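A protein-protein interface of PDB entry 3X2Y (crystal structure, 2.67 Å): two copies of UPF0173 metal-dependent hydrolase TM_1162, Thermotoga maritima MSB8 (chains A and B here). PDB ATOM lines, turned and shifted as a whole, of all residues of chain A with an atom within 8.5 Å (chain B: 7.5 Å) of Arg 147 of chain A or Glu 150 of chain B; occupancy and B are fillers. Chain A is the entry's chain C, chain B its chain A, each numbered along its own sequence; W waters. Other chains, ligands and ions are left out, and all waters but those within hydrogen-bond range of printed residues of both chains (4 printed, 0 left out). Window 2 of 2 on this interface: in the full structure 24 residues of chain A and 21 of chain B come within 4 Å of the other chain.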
ATOM      1  N   PRO A 106     -28.767  -0.776 -27.890  1.00  0.00           N
ATOM      2  CA  PRO A 106     -29.273  -1.686 -26.865  1.00  0.00           C
ATOM      3  C   PRO A 106     -30.620  -1.255 -26.296  1.00  0.00           C
ATOM      4  O   PRO A 106     -30.935  -0.062 -26.247  1.00  0.00           O
ATOM      5  CB  PRO A 106     -28.200  -1.630 -25.768  1.00  0.00           C
ATOM      6  CG  PRO A 106     -26.977  -1.127 -26.446  1.00  0.00           C
ATOM      7  CD  PRO A 106     -27.462  -0.207 -27.521  1.00  0.00           C
ATOM      8  N   VAL A 108     -33.530  -2.792 -23.057  1.00  0.00           N
ATOM      9  CA  VAL A 108     -33.841  -3.790 -22.047  1.00  0.00           C
ATOM     10  C   VAL A 108     -35.333  -4.062 -22.137  1.00  0.00           C
ATOM     11  O   VAL A 108     -36.153  -3.233 -21.757  1.00  0.00           O
ATOM     12  CB  VAL A 108     -33.371  -3.384 -20.632  1.00  0.00           C
ATOM     13  CG1 VAL A 108     -31.858  -3.241 -20.616  1.00  0.00           C
ATOM     14  CG2 VAL A 108     -34.024  -2.096 -20.151  1.00  0.00           C
ATOM     15  N   THR A 143     -38.374  -0.200 -24.318  1.00  0.00           N
ATOM     16  CA  THR A 143     -37.258  -0.380 -23.410  1.00  0.00           C
ATOM     17  C   THR A 143     -37.549   0.224 -22.043  1.00  0.00           C
ATOM     18  O   THR A 143     -38.378   1.126 -21.906  1.00  0.00           O
ATOM     19  CB  THR A 143     -35.958   0.238 -23.963  1.00  0.00           C
ATOM     20  OG1 THR A 143     -34.855  -0.102 -23.110  1.00  0.00           O
ATOM     21  CG2 THR A 143     -36.069   1.759 -24.075  1.00  0.00           C
ATOM     22  N   GLY A 144     -36.878  -0.319 -21.034  1.00  0.00           N
ATOM     23  CA  GLY A 144     -36.811   0.296 -19.733  1.00  0.00           C
ATOM     24  C   GLY A 144     -35.622   1.231 -19.690  1.00  0.00           C
ATOM     25  O   GLY A 144     -34.882   1.357 -20.666  1.00  0.00           O
ATOM     26  N   LEU A 145     -35.445   1.889 -18.556  1.00  0.00           N
ATOM     27  CA  LEU A 145     -34.282   2.728 -18.341  1.00  0.00           C
ATOM     28  C   LEU A 145     -33.037   1.848 -18.296  1.00  0.00           C
ATOM     29  O   LEU A 145     -33.018   0.819 -17.630  1.00  0.00           O
ATOM     30  CB  LEU A 145     -34.428   3.525 -17.041  1.00  0.00           C
ATOM     31  CG  LEU A 145     -33.306   4.499 -16.706  1.00  0.00           C
ATOM     32  CD1 LEU A 145     -33.206   5.598 -17.752  1.00  0.00           C
ATOM     33  CD2 LEU A 145     -33.513   5.088 -15.316  1.00  0.00           C
ATOM     34  N   THR A 146     -32.013   2.250 -19.036  1.00  0.00           N
ATOM     35  CA  THR A 146     -30.752   1.527 -19.071  1.00  0.00           C
ATOM     36  C   THR A 146     -29.611   2.525 -19.183  1.00  0.00           C
ATOM     37  O   THR A 146     -29.746   3.570 -19.825  1.00  0.00           O
ATOM     38  CB  THR A 146     -30.697   0.505 -20.235  1.00  0.00           C
ATOM     39  OG1 THR A 146     -29.371  -0.016 -20.366  1.00  0.00           O
ATOM     40  CG2 THR A 146     -31.104   1.132 -21.566  1.00  0.00           C
ATOM     41  N   ARG A 147     -28.487   2.190 -18.559  1.00  0.00           N
ATOM     42  CA  ARG A 147     -27.294   3.029 -18.603  1.00  0.00           C
ATOM     43  C   ARG A 147     -26.620   3.033 -19.977  1.00  0.00           C
ATOM     44  O   ARG A 147     -25.769   3.877 -20.242  1.00  0.00           O
ATOM     45  CB  ARG A 147     -26.296   2.587 -17.534  1.00  0.00           C
ATOM     46  CG  ARG A 147     -26.861   2.648 -16.123  1.00  0.00           C
ATOM     47  CD  ARG A 147     -25.763   2.878 -15.106  1.00  0.00           C
ATOM     48  NE  ARG A 147     -25.297   4.259 -15.144  1.00  0.00           N
ATOM     49  CZ  ARG A 147     -24.186   4.697 -14.562  1.00  0.00           C
ATOM     50  NH1 ARG A 147     -23.393   3.866 -13.888  1.00  0.00           N
ATOM     51  NH2 ARG A 147     -23.861   5.983 -14.663  1.00  0.00           N
ATOM     52  N   GLU A 148     -27.007   2.108 -20.849  1.00  0.00           N
ATOM     53  CA  GLU A 148     -26.525   2.120 -22.230  1.00  0.00           C
ATOM     54  C   GLU A 148     -26.945   3.391 -22.968  1.00  0.00           C
ATOM     55  O   GLU A 148     -26.280   3.796 -23.922  1.00  0.00           O
ATOM     56  CB  GLU A 148     -27.042   0.913 -23.020  1.00  0.00           C
ATOM     57  CG  GLU A 148     -26.789  -0.452 -22.399  1.00  0.00           C
ATOM     58  CD  GLU A 148     -25.323  -0.802 -22.254  1.00  0.00           C
ATOM     59  OE1 GLU A 148     -24.443   0.003 -22.629  1.00  0.00           O
ATOM     60  OE2 GLU A 148     -25.051  -1.905 -21.747  1.00  0.00           O
ATOM     61  N   MET A 149     -28.048   4.007 -22.541  1.00  0.00           N
ATOM     62  CA  MET A 149     -28.519   5.251 -23.149  1.00  0.00           C
ATOM     63  C   MET A 149     -27.499   6.385 -23.047  1.00  0.00           C
ATOM     64  O   MET A 149     -27.479   7.262 -23.905  1.00  0.00           O
ATOM     65  CB  MET A 149     -29.854   5.691 -22.532  1.00  0.00           C
ATOM     66  CG  MET A 149     -31.040   4.849 -22.969  1.00  0.00           C
ATOM     67  SD  MET A 149     -32.473   5.054 -21.892  1.00  0.00           S
ATOM     68  CE  MET A 149     -33.672   4.024 -22.727  1.00  0.00           C
ATOM     69  N   GLU A 150     -26.657   6.361 -22.012  1.00  0.00           N
ATOM     70  CA  GLU A 150     -25.600   7.364 -21.847  1.00  0.00           C
ATOM     71  C   GLU A 150     -24.576   7.352 -22.997  1.00  0.00           C
ATOM     72  O   GLU A 150     -23.920   8.360 -23.251  1.00  0.00           O
ATOM     73  CB  GLU A 150     -24.888   7.184 -20.501  1.00  0.00           C
ATOM     74  CG  GLU A 150     -25.750   7.525 -19.291  1.00  0.00           C
ATOM     75  CD  GLU A 150     -25.254   6.904 -17.983  1.00  0.00           C
ATOM     76  OE1 GLU A 150     -24.716   5.770 -18.008  1.00  0.00           O
ATOM     77  OE2 GLU A 150     -25.418   7.541 -16.918  1.00  0.00           O
ATOM     78  N   LEU A 151     -24.448   6.226 -23.693  1.00  0.00           N
ATOM     79  CA  LEU A 151     -23.577   6.141 -24.874  1.00  0.00           C
ATOM     80  C   LEU A 151     -24.003   7.099 -25.996  1.00  0.00           C
ATOM     81  O   LEU A 151     -23.173   7.527 -26.801  1.00  0.00           O
ATOM     82  CB  LEU A 151     -23.553   4.712 -25.429  1.00  0.00           C
ATOM     83  CG  LEU A 151     -23.023   3.614 -24.503  1.00  0.00           C
ATOM     84  CD1 LEU A 151     -23.216   2.242 -25.133  1.00  0.00           C
ATOM     85  CD2 LEU A 151     -21.564   3.854 -24.153  1.00  0.00           C
ATOM     86  N   LEU A 152     -25.296   7.419 -26.040  1.00  0.00           N
ATOM     87  CA  LEU A 152     -25.857   8.296 -27.062  1.00  0.00           C
ATOM     88  C   LEU A 152     -25.650   9.788 -26.792  1.00  0.00           C
ATOM     89  O   LEU A 152     -25.855  10.600 -27.682  1.00  0.00           O
ATOM     90  CB  LEU A 152     -27.355   8.013 -27.219  1.00  0.00           C
ATOM     91  CG  LEU A 152     -27.740   6.590 -27.628  1.00  0.00           C
ATOM     92  CD1 LEU A 152     -29.236   6.386 -27.484  1.00  0.00           C
ATOM     93  CD2 LEU A 152     -27.300   6.287 -29.050  1.00  0.00           C
ATOM     94  N   ALA A 153     -25.247  10.155 -25.578  1.00  0.00           N
ATOM     95  CA  ALA A 153     -25.052  11.568 -25.225  1.00  0.00           C
ATOM     96  C   ALA A 153     -24.083  12.277 -26.167  1.00  0.00           C
ATOM     97  O   ALA A 153     -24.350  13.399 -26.602  1.00  0.00           O
ATOM     98  CB  ALA A 153     -24.571  11.702 -23.788  1.00  0.00           C
ATOM     99  N   ARG A 177     -35.486  10.499 -16.745  1.00  0.00           N
ATOM    100  CA  ARG A 177     -34.109  10.077 -16.478  1.00  0.00           C
ATOM    101  C   ARG A 177     -33.379   9.662 -17.759  1.00  0.00           C
ATOM    102  O   ARG A 177     -32.190   9.946 -17.911  1.00  0.00           O
ATOM    103  CB  ARG A 177     -34.071   8.936 -15.444  1.00  0.00           C
ATOM    104  CG  ARG A 177     -34.500   9.355 -14.038  1.00  0.00           C
ATOM    105  CD  ARG A 177     -34.788   8.163 -13.124  1.00  0.00           C
ATOM    106  NE  ARG A 177     -33.571   7.479 -12.677  1.00  0.00           N
ATOM    107  CZ  ARG A 177     -33.542   6.295 -12.060  1.00  0.00           C
ATOM    108  NH1 ARG A 177     -34.658   5.625 -11.800  1.00  0.00           N
ATOM    109  NH2 ARG A 177     -32.377   5.770 -11.699  1.00  0.00           N
ATOM    110  N   ALA A 178     -34.083   8.998 -18.677  1.00  0.00           N
ATOM    111  CA  ALA A 178     -33.485   8.623 -19.970  1.00  0.00           C
ATOM    112  C   ALA A 178     -33.140   9.853 -20.814  1.00  0.00           C
ATOM    113  O   ALA A 178     -32.064   9.921 -21.406  1.00  0.00           O
ATOM    114  CB  ALA A 178     -34.402   7.703 -20.751  1.00  0.00           C
ATOM    115  N   MET A 181     -29.984  11.363 -19.622  1.00  0.00           N
ATOM    116  CA  MET A 181     -28.844  10.554 -20.058  1.00  0.00           C
ATOM    117  C   MET A 181     -28.491  10.834 -21.514  1.00  0.00           C
ATOM    118  O   MET A 181     -27.320  10.941 -21.868  1.00  0.00           O
ATOM    119  CB  MET A 181     -29.142   9.062 -19.942  1.00  0.00           C
ATOM    120  CG  MET A 181     -29.074   8.479 -18.548  1.00  0.00           C
ATOM    121  SD  MET A 181     -29.475   6.720 -18.606  1.00  0.00           S
ATOM    122  CE  MET A 181     -29.381   6.318 -16.863  1.00  0.00           C
ATOM    123  N   ILE A 182     -29.514  10.919 -22.358  1.00  0.00           N
ATOM    124  CA  ILE A 182     -29.320  11.062 -23.799  1.00  0.00           C
ATOM    125  C   ILE A 182     -29.004  12.508 -24.188  1.00  0.00           C
ATOM    126  O   ILE A 182     -28.219  12.738 -25.099  1.00  0.00           O
ATOM    127  CB  ILE A 182     -30.545  10.537 -24.578  1.00  0.00           C
ATOM    128  CG1 ILE A 182     -30.757   9.045 -24.282  1.00  0.00           C
ATOM    129  CG2 ILE A 182     -30.356  10.734 -26.075  1.00  0.00           C
ATOM    130  CD1 ILE A 182     -32.158   8.550 -24.567  1.00  0.00           C
ATOM    131  N   PRO B 106     -33.571  -4.820 -14.813  1.00  0.00           N
ATOM    132  CA  PRO B 106     -32.729  -5.597 -15.719  1.00  0.00           C
ATOM    133  C   PRO B 106     -31.865  -6.651 -15.004  1.00  0.00           C
ATOM    134  O   PRO B 106     -31.525  -6.499 -13.836  1.00  0.00           O
ATOM    135  CB  PRO B 106     -31.847  -4.533 -16.389  1.00  0.00           C
ATOM    136  CG  PRO B 106     -32.503  -3.227 -16.099  1.00  0.00           C
ATOM    137  CD  PRO B 106     -33.192  -3.400 -14.789  1.00  0.00           C
ATOM    138  N   THR B 146     -23.982  -6.340 -13.079  1.00  0.00           N
ATOM    139  CA  THR B 146     -24.304  -5.439 -14.188  1.00  0.00           C
ATOM    140  C   THR B 146     -24.361  -4.000 -13.708  1.00  0.00           C
ATOM    141  O   THR B 146     -24.834  -3.733 -12.610  1.00  0.00           O
ATOM    142  CB  THR B 146     -25.649  -5.790 -14.860  1.00  0.00           C
ATOM    143  OG1 THR B 146     -26.077  -4.694 -15.672  1.00  0.00           O
ATOM    144  CG2 THR B 146     -26.734  -6.078 -13.842  1.00  0.00           C
ATOM    145  N   ARG B 147     -23.897  -3.079 -14.549  1.00  0.00           N
ATOM    146  CA  ARG B 147     -23.918  -1.645 -14.245  1.00  0.00           C
ATOM    147  C   ARG B 147     -25.333  -1.070 -14.106  1.00  0.00           C
ATOM    148  O   ARG B 147     -25.505   0.015 -13.569  1.00  0.00           O
ATOM    149  CB  ARG B 147     -23.147  -0.854 -15.308  1.00  0.00           C
ATOM    150  CG  ARG B 147     -21.673  -1.219 -15.408  1.00  0.00           C
ATOM    151  CD  ARG B 147     -20.840  -0.007 -15.783  1.00  0.00           C
ATOM    152  NE  ARG B 147     -20.668   0.877 -14.636  1.00  0.00           N
ATOM    153  CZ  ARG B 147     -20.242   2.135 -14.695  1.00  0.00           C
ATOM    154  NH1 ARG B 147     -19.940   2.702 -15.854  1.00  0.00           N
ATOM    155  NH2 ARG B 147     -20.128   2.836 -13.574  1.00  0.00           N
ATOM    156  N   GLU B 148     -26.339  -1.794 -14.595  1.00  0.00           N
ATOM    157  CA  GLU B 148     -27.738  -1.409 -14.401  1.00  0.00           C
ATOM    158  C   GLU B 148     -28.132  -1.347 -12.930  1.00  0.00           C
ATOM    159  O   GLU B 148     -29.077  -0.640 -12.574  1.00  0.00           O
ATOM    160  CB  GLU B 148     -28.684  -2.385 -15.112  1.00  0.00           C
ATOM    161  CG  GLU B 148     -28.491  -2.531 -16.617  1.00  0.00           C
ATOM    162  CD  GLU B 148     -28.509  -1.208 -17.372  1.00  0.00           C
ATOM    163  OE1 GLU B 148     -29.065  -0.210 -16.858  1.00  0.00           O
ATOM    164  OE2 GLU B 148     -27.958  -1.165 -18.492  1.00  0.00           O
ATOM    165  N   MET B 149     -27.427  -2.092 -12.081  1.00  0.00           N
ATOM    166  CA  MET B 149     -27.702  -2.093 -10.644  1.00  0.00           C
ATOM    167  C   MET B 149     -27.476  -0.734  -9.986  1.00  0.00           C
ATOM    168  O   MET B 149     -28.114  -0.424  -8.982  1.00  0.00           O
ATOM    169  CB  MET B 149     -26.852  -3.152  -9.941  1.00  0.00           C
ATOM    170  CG  MET B 149     -27.296  -4.575 -10.223  1.00  0.00           C
ATOM    171  SD  MET B 149     -26.011  -5.760  -9.805  1.00  0.00           S
ATOM    172  CE  MET B 149     -26.896  -7.317  -9.919  1.00  0.00           C
ATOM    173  N   GLU B 150     -26.584   0.078 -10.558  1.00  0.00           N
ATOM    174  CA  GLU B 150     -26.333   1.429 -10.054  1.00  0.00           C
ATOM    175  C   GLU B 150     -27.601   2.288 -10.089  1.00  0.00           C
ATOM    176  O   GLU B 150     -27.741   3.212  -9.293  1.00  0.00           O
ATOM    177  CB  GLU B 150     -25.204   2.108 -10.840  1.00  0.00           C
ATOM    178  CG  GLU B 150     -23.802   1.793 -10.326  1.00  0.00           C
ATOM    179  CD  GLU B 150     -22.710   1.864 -11.397  1.00  0.00           C
ATOM    180  OE1 GLU B 150     -23.016   1.712 -12.599  1.00  0.00           O
ATOM    181  OE2 GLU B 150     -21.527   2.057 -11.040  1.00  0.00           O
ATOM    182  N   LEU B 151     -28.526   1.972 -10.992  1.00  0.00           N
ATOM    183  CA  LEU B 151     -29.792   2.699 -11.087  1.00  0.00           C
ATOM    184  C   LEU B 151     -30.664   2.572  -9.829  1.00  0.00           C
ATOM    185  O   LEU B 151     -31.515   3.427  -9.587  1.00  0.00           O
ATOM    186  CB  LEU B 151     -30.598   2.231 -12.306  1.00  0.00           C
ATOM    187  CG  LEU B 151     -29.948   2.400 -13.683  1.00  0.00           C
ATOM    188  CD1 LEU B 151     -30.793   1.715 -14.750  1.00  0.00           C
ATOM    189  CD2 LEU B 151     -29.723   3.864 -14.019  1.00  0.00           C
ATOM    190  N   LEU B 152     -30.449   1.512  -9.046  1.00  0.00           N
ATOM    191  CA  LEU B 152     -31.229   1.251  -7.839  1.00  0.00           C
ATOM    192  C   LEU B 152     -30.739   2.007  -6.609  1.00  0.00           C
ATOM    193  O   LEU B 152     -31.425   2.021  -5.589  1.00  0.00           O
ATOM    194  CB  LEU B 152     -31.232  -0.251  -7.527  1.00  0.00           C
ATOM    195  CG  LEU B 152     -31.774  -1.178  -8.615  1.00  0.00           C
ATOM    196  CD1 LEU B 152     -31.586  -2.633  -8.213  1.00  0.00           C
ATOM    197  CD2 LEU B 152     -33.238  -0.893  -8.913  1.00  0.00           C
ATOM    198  N   ALA B 153     -29.561   2.621  -6.677  1.00  0.00           N
ATOM    199  CA  ALA B 153     -29.017   3.331  -5.512  1.00  0.00           C
ATOM    200  C   ALA B 153     -29.970   4.425  -5.034  1.00  0.00           C
ATOM    201  O   ALA B 153     -30.187   4.580  -3.830  1.00  0.00           O
ATOM    202  CB  ALA B 153     -27.644   3.917  -5.817  1.00  0.00           C
ATOM    203  N   GLU B 154     -30.549   5.168  -5.974  1.00  0.00           N
ATOM    204  CA  GLU B 154     -31.462   6.255  -5.629  1.00  0.00           C
ATOM    205  C   GLU B 154     -32.808   5.778  -5.053  1.00  0.00           C
ATOM    206  O   GLU B 154     -33.540   6.566  -4.458  1.00  0.00           O
ATOM    207  CB  GLU B 154     -31.685   7.182  -6.829  1.00  0.00           C
ATOM    208  CG  GLU B 154     -32.492   6.597  -7.978  1.00  0.00           C
ATOM    209  CD  GLU B 154     -33.009   7.679  -8.907  1.00  0.00           C
ATOM    210  OE1 GLU B 154     -32.203   8.542  -9.325  1.00  0.00           O
ATOM    211  OE2 GLU B 154     -34.225   7.680  -9.205  1.00  0.00           O
ATOM    212  N   GLU B 155     -33.122   4.497  -5.226  1.00  0.00           N
ATOM    213  CA  GLU B 155     -34.326   3.903  -4.643  1.00  0.00           C
ATOM    214  C   GLU B 155     -34.228   3.714  -3.128  1.00  0.00           C
ATOM    215  O   GLU B 155     -35.244   3.625  -2.458  1.00  0.00           O
ATOM    216  CB  GLU B 155     -34.623   2.547  -5.290  1.00  0.00           C
ATOM    217  CG  GLU B 155     -34.890   2.600  -6.786  1.00  0.00           C
ATOM    218  CD  GLU B 155     -36.179   3.323  -7.134  1.00  0.00           C
ATOM    219  OE1 GLU B 155     -37.021   3.525  -6.227  1.00  0.00           O
ATOM    220  OE2 GLU B 155     -36.350   3.684  -8.324  1.00  0.00           O
ATOM    221  N   ARG B 177     -19.531  -6.273  -4.926  1.00  0.00           N
ATOM    222  CA  ARG B 177     -19.524  -5.131  -5.832  1.00  0.00           C
ATOM    223  C   ARG B 177     -20.945  -4.672  -6.153  1.00  0.00           C
ATOM    224  O   ARG B 177     -21.185  -3.480  -6.322  1.00  0.00           O
ATOM    225  CB  ARG B 177     -18.776  -5.468  -7.123  1.00  0.00           C
ATOM    226  CG  ARG B 177     -17.275  -5.627  -6.953  1.00  0.00           C
ATOM    227  CD  ARG B 177     -16.635  -6.266  -8.175  1.00  0.00           C
ATOM    228  NE  ARG B 177     -16.519  -5.352  -9.316  1.00  0.00           N
ATOM    229  CZ  ARG B 177     -16.143  -5.714 -10.550  1.00  0.00           C
ATOM    230  NH1 ARG B 177     -15.850  -6.985 -10.829  1.00  0.00           N
ATOM    231  NH2 ARG B 177     -16.065  -4.805 -11.517  1.00  0.00           N
ATOM    232  N   ALA B 178     -21.881  -5.614  -6.246  1.00  0.00           N
ATOM    233  CA  ALA B 178     -23.278  -5.275  -6.503  1.00  0.00           C
ATOM    234  C   ALA B 178     -23.915  -4.577  -5.311  1.00  0.00           C
ATOM    235  O   ALA B 178     -24.709  -3.663  -5.487  1.00  0.00           O
ATOM    236  CB  ALA B 178     -24.077  -6.509  -6.870  1.00  0.00           C
ATOM    237  N   VAL B 180     -22.357  -2.684  -3.188  1.00  0.00           N
ATOM    238  CA  VAL B 180     -21.798  -1.329  -3.164  1.00  0.00           C
ATOM    239  C   VAL B 180     -22.436  -0.430  -4.238  1.00  0.00           C
ATOM    240  O   VAL B 180     -22.528   0.787  -4.059  1.00  0.00           O
ATOM    241  CB  VAL B 180     -20.264  -1.370  -3.320  1.00  0.00           C
ATOM    242  CG1 VAL B 180     -19.676   0.028  -3.458  1.00  0.00           C
ATOM    243  CG2 VAL B 180     -19.643  -2.075  -2.122  1.00  0.00           C
ATOM    244  N   MET B 181     -22.870  -1.031  -5.346  1.00  0.00           N
ATOM    245  CA  MET B 181     -23.601  -0.303  -6.378  1.00  0.00           C
ATOM    246  C   MET B 181     -25.016   0.055  -5.926  1.00  0.00           C
ATOM    247  O   MET B 181     -25.481   1.165  -6.168  1.00  0.00           O
ATOM    248  CB  MET B 181     -23.688  -1.126  -7.663  1.00  0.00           C
ATOM    249  CG  MET B 181     -22.382  -1.212  -8.434  1.00  0.00           C
ATOM    250  SD  MET B 181     -22.437  -2.393  -9.796  1.00  0.00           S
ATOM    251  CE  MET B 181     -23.644  -1.621 -10.825  1.00  0.00           C
ATOM    252  N   ILE B 182     -25.694  -0.892  -5.282  1.00  0.00           N
ATOM    253  CA  ILE B 182     -27.088  -0.732  -4.879  1.00  0.00           C
ATOM    254  C   ILE B 182     -27.212   0.028  -3.554  1.00  0.00           C
ATOM    255  O   ILE B 182     -28.124   0.825  -3.374  1.00  0.00           O
ATOM    256  CB  ILE B 182     -27.777  -2.108  -4.762  1.00  0.00           C
ATOM    257  CG1 ILE B 182     -27.759  -2.833  -6.119  1.00  0.00           C
ATOM    258  CG2 ILE B 182     -29.213  -1.963  -4.267  1.00  0.00           C
ATOM    259  CD1 ILE B 182     -27.979  -4.333  -6.022  1.00  0.00           C
HETATM  260  O   HOH W   1     -30.134   7.098 -10.662  1.00  0.00           O
HETATM  261  O   HOH W   2     -25.402  -1.682 -19.082  1.00  0.00           O
HETATM  262  O   HOH W   3     -32.052  10.368 -11.585  1.00  0.00           O
HETATM  263  O   HOH W   4     -34.138   3.319  -9.993  1.00  0.00           O
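Water W4 lies within hydrogen-bond range of the backbone carbonyl oxygen of Leu 151 of chain B, the side-chain carboxylate of Glu 155 of chain B and the guanidinium group of Arg 177 of chain A. Water W2 bridges the side-chain carboxylate (OE2) of Glu 148 of chain B (2.7 Å) and the side-chain carboxylate (OE2) of Glu 148 of chain A (2.7 Å). Water W1 lies within hydrogen-bond range of NH2 of Arg 177 of chain A and OE1 of Glu 154 of chain B. Water W3 lies within hydrogen-bond range of the side-chain carboxylate of Glu 154 of chain B and the guanidinium group of Arg 177 of chain A.
Printed residues of chain A that touch a printed residue of chain B: Leu 145, Thr 146, Arg 147, Arg 177 and Met 181. Hydrophobic or aromatic side chains of chain A within 4 Å of the printed part of chain B: Met 181. Hydrophobic or aromatic side chains of chain B within 4 Å of the printed part of chain A: Leu 151. Among the printed residues, Asp or Glu carboxylates within 4 Å of a Lys or Arg side-chain nitrogen of the other chain: Arg 147 of chain A with Glu 150 of chain B (2.5 Å) and Arg 177 of chain A with Glu 154 of chain B (3.3 Å).
Arg 147 of chain A touches just these residues of chain B: Arg 147 (3.3 Å), Glu 148 (3.0 Å), Glu 150 (2.5 Å) and Leu 151 (3.8 Å). Of the printed residues of chain A, Glu 150 of chain B touches Arg 147 (2.5 Å). Leu 151 of chain B touches just these residues of chain A: Leu 145, Arg 147, Arg 177 and Met 181. Of the printed residues of chain B, Met 181 of chain A touches Leu 151 (3.8 Å). Of the printed residues of chain B, Arg 177 of chain A touches Leu 151 (3.3 Å) and Glu 154 (3.2 Å). Of the printed residues of chain A, Glu 148 of chain B touches Thr 146 (2.6 Å) and Arg 147 (3.0 Å). Of the printed residues of chain A, Arg 147 of chain B touches Arg 147. Printed residues of chain B within 4 Å of Leu 145 of chain A: Leu 151 (3.7 Å). Glu 150 of chain A touches none of the printed residues of chain B. The nearest printed residue of chain B that does not touch Thr 146 of chain A is Leu 151 of chain B (4.3 Å).
The backbone NH (N) of Glu 148 of chain B sits close to the side-chain hydroxyl (OG1) of Thr 146 of chain B (3.1 Å). OE2 of Glu 150 of chain B is in salt-bridge range of NH2 of Arg 147 of chain B (3.0 Å). The backbone NH (N) of Glu 148 of chain A sits close to the side-chain hydroxyl (OG1) of Thr 146 of chain A. NH2 of Arg 147 of chain A is in salt-bridge range of OE2 of Glu 150 of chain A (3.2 Å).
Arg 147 of chain A touches Glu 150 of chain B, but with the chains exchanged Glu 150 of chain A does not touch Arg 147 of chain B (6.1 Å). Arg 147 of chain A touches Leu 151 of chain B, but with the chains exchanged Leu 151 of chain A does not touch Arg 147 of chain B (8.5 Å). Arg 177 of chain A touches Leu 151 of chain B, but with the chains exchanged Leu 151 of chain A does not touch Arg 177 of chain B (16.3 Å). Met 181 of chain A touches Leu 151 of chain B, but with the chains exchanged Leu 151 of chain A does not touch Met 181 of chain B (14.6 Å). Positions printed for both chains: 106, 146, 147, 148, 149, 150, 151, 152, 153, 177, 178, 181 and 182.
Leu 145 of chain A touches Leu 151 of chain B. Leu 151 of chain B touches Arg 147 of chain A. Leu 151 of chain B touches Met 181 of chain A (CD2 to CE, 3.8 Å).
The side-chain carboxylate of Glu 148 of chain B lies within hydrogen-bond range of the side-chain hydroxyl of Thr 146 of chain A (2.6 Å). OE1 of Glu 148 of chain B lies within hydrogen-bond range of N of Arg 147 of chain A. OE1 of Glu 150 of chain B is in salt-bridge range of NH1 of Arg 147 of chain A (2.5 Å). NH2 of Arg 177 of chain A is in hydrogen-bond range of O of Leu 151 of chain B. The side-chain carboxylate (OE2) of Glu 154 of chain B lies within salt-bridge range of the guanidinium group (NH1) of Arg 177 of chain A, 3.3 Å away. NH1 of Arg 147 of chain A lies close to NH2 of Arg 147 of chain B (3.4 Å).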
